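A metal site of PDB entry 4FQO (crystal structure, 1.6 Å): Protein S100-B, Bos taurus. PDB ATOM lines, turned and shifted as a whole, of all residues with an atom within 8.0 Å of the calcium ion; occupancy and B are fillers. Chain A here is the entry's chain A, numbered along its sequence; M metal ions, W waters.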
ATOM      1  N   LYS A  27      11.576 -13.186 -12.239  1.00  0.00           N
ATOM      2  CA  LYS A  27      12.519 -12.133 -11.844  1.00  0.00           C
ATOM      3  C   LYS A  27      11.911 -10.764 -12.104  1.00  0.00           C
ATOM      4  O   LYS A  27      11.046 -10.598 -12.984  1.00  0.00           O
ATOM      5  CB  LYS A  27      13.844 -12.253 -12.616  1.00  0.00           C
ATOM      6  CG  LYS A  27      14.570 -13.605 -12.457  1.00  0.00           C
ATOM      7  CD  LYS A  27      15.845 -13.611 -13.266  1.00  0.00           C
ATOM      8  CE  LYS A  27      16.563 -14.933 -13.147  1.00  0.00           C
ATOM      9  NZ  LYS A  27      17.681 -14.935 -14.168  1.00  0.00           N
ATOM     10  N   LEU A  28      12.370  -9.769 -11.346  1.00  0.00           N
ATOM     11  CA  LEU A  28      11.992  -8.379 -11.559  1.00  0.00           C
ATOM     12  C   LEU A  28      13.054  -7.731 -12.435  1.00  0.00           C
ATOM     13  O   LEU A  28      14.197  -7.574 -12.007  1.00  0.00           O
ATOM     14  CB  LEU A  28      11.924  -7.609 -10.247  1.00  0.00           C
ATOM     15  CG  LEU A  28      10.899  -8.105  -9.216  1.00  0.00           C
ATOM     16  CD1 LEU A  28      11.296  -7.583  -7.802  1.00  0.00           C
ATOM     17  CD2 LEU A  28       9.504  -7.669  -9.565  1.00  0.00           C
ATOM     18  N   MET A  58      18.951  -1.335  -8.800  1.00  0.00           N
ATOM     19  CA  MET A  58      19.251  -2.647  -9.357  1.00  0.00           C
ATOM     20  C   MET A  58      20.714  -3.045  -9.169  1.00  0.00           C
ATOM     21  O   MET A  58      21.004  -4.194  -8.875  1.00  0.00           O
ATOM     22  CB  MET A  58      18.831  -2.756 -10.836  1.00  0.00           C
ATOM     23  CG  MET A  58      18.905  -4.190 -11.400  1.00  0.00           C
ATOM     24  SD  MET A  58      17.807  -5.405 -10.605  1.00  0.00           S
ATOM     25  CE  MET A  58      16.286  -5.076 -11.497  1.00  0.00           C
ATOM     26  N   LEU A  61      21.066  -4.415  -5.786  1.00  0.00           N
ATOM     27  CA  LEU A  61      20.311  -5.647  -5.564  1.00  0.00           C
ATOM     28  C   LEU A  61      20.806  -6.847  -6.354  1.00  0.00           C
ATOM     29  O   LEU A  61      20.639  -7.994  -5.909  1.00  0.00           O
ATOM     30  CB  LEU A  61      18.825  -5.438  -5.862  1.00  0.00           C
ATOM     31  CG  LEU A  61      18.063  -4.462  -4.994  1.00  0.00           C
ATOM     32  CD1 LEU A  61      16.592  -4.658  -5.331  1.00  0.00           C
ATOM     33  CD2 LEU A  61      18.342  -4.739  -3.506  1.00  0.00           C
ATOM     34  N   ASP A  62      21.402  -6.594  -7.521  1.00  0.00           N
ATOM     35  CA  ASP A  62      21.675  -7.680  -8.463  1.00  0.00           C
ATOM     36  C   ASP A  62      23.011  -8.380  -8.182  1.00  0.00           C
ATOM     37  O   ASP A  62      24.022  -7.989  -8.716  1.00  0.00           O
ATOM     38  CB  ASP A  62      21.580  -7.144  -9.906  1.00  0.00           C
ATOM     39  CG  ASP A  62      21.928  -8.186 -10.931  1.00  0.00           C
ATOM     40  OD1 ASP A  62      21.706  -9.382 -10.649  1.00  0.00           O
ATOM     41  OD2 ASP A  62      22.441  -7.791 -12.007  1.00  0.00           O
ATOM     42  N   SER A  63      23.007  -9.427  -7.370  1.00  0.00           N
ATOM     43  CA  SER A  63      24.267 -10.035  -6.938  1.00  0.00           C
ATOM     44  C   SER A  63      24.836 -11.047  -7.937  1.00  0.00           C
ATOM     45  O   SER A  63      25.959 -11.482  -7.786  1.00  0.00           O
ATOM     46  CB  SER A  63      24.124 -10.696  -5.567  1.00  0.00           C
ATOM     47  OG  SER A  63      23.652  -9.745  -4.627  1.00  0.00           O
ATOM     48  N   ASP A  64      24.060 -11.449  -8.938  1.00  0.00           N
ATOM     49  CA  ASP A  64      24.592 -12.412  -9.899  1.00  0.00           C
ATOM     50  C   ASP A  64      24.782 -11.840 -11.287  1.00  0.00           C
ATOM     51  O   ASP A  64      25.077 -12.567 -12.227  1.00  0.00           O
ATOM     52  CB  ASP A  64      23.783 -13.738  -9.913  1.00  0.00           C
ATOM     53  CG  ASP A  64      22.357 -13.554 -10.407  1.00  0.00           C
ATOM     54  OD1 ASP A  64      21.984 -12.424 -10.742  1.00  0.00           O
ATOM     55  OD2 ASP A  64      21.596 -14.556 -10.394  1.00  0.00           O
ATOM     56  N   GLY A  65      24.594 -10.522 -11.407  1.00  0.00           N
ATOM     57  CA  GLY A  65      24.979  -9.807 -12.596  1.00  0.00           C
ATOM     58  C   GLY A  65      24.128 -10.010 -13.839  1.00  0.00           C
ATOM     59  O   GLY A  65      24.587  -9.715 -14.958  1.00  0.00           O
ATOM     60  N   ASP A  66      22.896 -10.497 -13.669  1.00  0.00           N
ATOM     61  CA  ASP A  66      21.996 -10.720 -14.833  1.00  0.00           C
ATOM     62  C   ASP A  66      21.090  -9.536 -15.157  1.00  0.00           C
ATOM     63  O   ASP A  66      20.278  -9.580 -16.108  1.00  0.00           O
ATOM     64  CB  ASP A  66      21.202 -12.025 -14.685  1.00  0.00           C
ATOM     65  CG  ASP A  66      20.128 -11.960 -13.640  1.00  0.00           C
ATOM     66  OD1 ASP A  66      20.064 -10.968 -12.878  1.00  0.00           O
ATOM     67  OD2 ASP A  66      19.328 -12.925 -13.550  1.00  0.00           O
ATOM     68  N   GLY A  67      21.245  -8.473 -14.379  1.00  0.00           N
ATOM     69  CA  GLY A  67      20.497  -7.256 -14.615  1.00  0.00           C
ATOM     70  C   GLY A  67      19.083  -7.248 -14.049  1.00  0.00           C
ATOM     71  O   GLY A  67      18.349  -6.267 -14.202  1.00  0.00           O
ATOM     72  N   GLU A  68      18.709  -8.351 -13.404  1.00  0.00           N
ATOM     73  CA  GLU A  68      17.379  -8.495 -12.818  1.00  0.00           C
ATOM     74  C   GLU A  68      17.459  -8.914 -11.369  1.00  0.00           C
ATOM     75  O   GLU A  68      18.517  -9.331 -10.869  1.00  0.00           O
ATOM     76  CB  GLU A  68      16.568  -9.518 -13.603  1.00  0.00           C
ATOM     77  CG  GLU A  68      16.469  -9.210 -15.094  1.00  0.00           C
ATOM     78  CD  GLU A  68      15.253  -9.774 -15.747  1.00  0.00           C
ATOM     79  OE1 GLU A  68      14.269 -10.034 -15.048  1.00  0.00           O
ATOM     80  OE2 GLU A  68      15.268  -9.927 -16.998  1.00  0.00           O
ATOM     81  N   CYS A  69      16.334  -8.785 -10.673  1.00  0.00           N
ATOM     82  CA  CYS A  69      16.292  -9.132  -9.254  1.00  0.00           C
ATOM     83  C   CYS A  69      15.445 -10.384  -9.083  1.00  0.00           C
ATOM     84  O   CYS A  69      14.230 -10.351  -9.312  1.00  0.00           O
ATOM     85  CB  CYS A  69      15.742  -7.949  -8.472  1.00  0.00           C
ATOM     86  SG  CYS A  69      15.469  -8.274  -6.695  1.00  0.00           S
ATOM     87  N   ASP A  70      16.095 -11.497  -8.714  1.00  0.00           N
ATOM     88  CA  ASP A  70      15.376 -12.760  -8.502  1.00  0.00           C
ATOM     89  C   ASP A  70      14.796 -12.823  -7.081  1.00  0.00           C
ATOM     90  O   ASP A  70      14.827 -11.825  -6.371  1.00  0.00           O
ATOM     91  CB  ASP A  70      16.238 -13.979  -8.878  1.00  0.00           C
ATOM     92  CG  ASP A  70      17.451 -14.170  -7.975  1.00  0.00           C
ATOM     93  OD1 ASP A  70      17.487 -13.626  -6.850  1.00  0.00           O
ATOM     94  OD2 ASP A  70      18.360 -14.935  -8.394  1.00  0.00           O
ATOM     95  N   PHE A  71      14.220 -13.962  -6.708  1.00  0.00           N
ATOM     96  CA  PHE A  71      13.535 -14.004  -5.430  1.00  0.00           C
ATOM     97  C   PHE A  71      14.503 -13.834  -4.237  1.00  0.00           C
ATOM     98  O   PHE A  71      14.218 -13.086  -3.305  1.00  0.00           O
ATOM     99  CB  PHE A  71      12.720 -15.274  -5.266  1.00  0.00           C
ATOM    100  CG  PHE A  71      11.821 -15.215  -4.073  1.00  0.00           C
ATOM    101  CD1 PHE A  71      10.618 -14.511  -4.115  1.00  0.00           C
ATOM    102  CD2 PHE A  71      12.178 -15.837  -2.892  1.00  0.00           C
ATOM    103  CE1 PHE A  71       9.782 -14.435  -3.002  1.00  0.00           C
ATOM    104  CE2 PHE A  71      11.321 -15.763  -1.771  1.00  0.00           C
ATOM    105  CZ  PHE A  71      10.144 -15.060  -1.835  1.00  0.00           C
ATOM    106  N   GLU A  73      17.351 -12.279  -4.281  1.00  0.00           N
ATOM    107  CA  GLU A  73      17.785 -10.866  -4.299  1.00  0.00           C
ATOM    108  C   GLU A  73      16.692  -9.949  -3.751  1.00  0.00           C
ATOM    109  O   GLU A  73      16.966  -8.956  -3.060  1.00  0.00           O
ATOM    110  CB  GLU A  73      18.287 -10.454  -5.691  1.00  0.00           C
ATOM    111  CG  GLU A  73      19.516 -11.245  -6.119  1.00  0.00           C
ATOM    112  CD  GLU A  73      19.785 -11.158  -7.604  1.00  0.00           C
ATOM    113  OE1 GLU A  73      18.828 -10.912  -8.375  1.00  0.00           O
ATOM    114  OE2 GLU A  73      20.957 -11.336  -7.995  1.00  0.00           O
HETATM  115 CA    CA M   1      20.158 -11.018 -10.471  1.00  0.00          CA
HETATM  116  O   HOH W   1      18.853 -12.817 -10.877  1.00  0.00           O
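OD2 of Asp 66 lies within salt-bridge range of NZ of Lys 27 (2.7 Å).
OE2 of Glu 73 sits close to N of Ser 63 (2.9 Å).
The backbone NH (N) of Glu 73 sits at hydrogen-bond distance from the side-chain carboxylate (OD1) of Asp 70, at 2.9 Å.
OD2 of Asp 62 sits at hydrogen-bond distance from N of Gly 67 (2.7 Å).
The side-chain carboxylate (OD1) of Asp 62 lies close to the backbone NH (N) of Gly 65, 3.2 Å away.
Within 4 Å of the calcium ion: Asp 62, Asp 64, Asp 66, Glu 68 and Glu 73.
Along chain A the residues within 4 Å of the calcium ion span positions 62 to 73.
The calcium ion is bound by OD1 of Asp 62.
The calcium ion is bound by water W1 (2.3 Å).
The calcium ion is bound by the side-chain carboxylate (OD1) of Asp 64 (2.3 Å).
The calcium ion is bound by O of Glu 68 (2.4 Å).
The calcium ion is bound by the side-chain carboxylate (OD1) of Asp 66.
The calcium ion is bound by the side-chain carboxylate (OE1) of Glu 73 (2.5 Å).
OE2 of Glu 73 is bound to the calcium ion (2.6 Å).
The calcium ion has seven donor atoms within binding distance.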
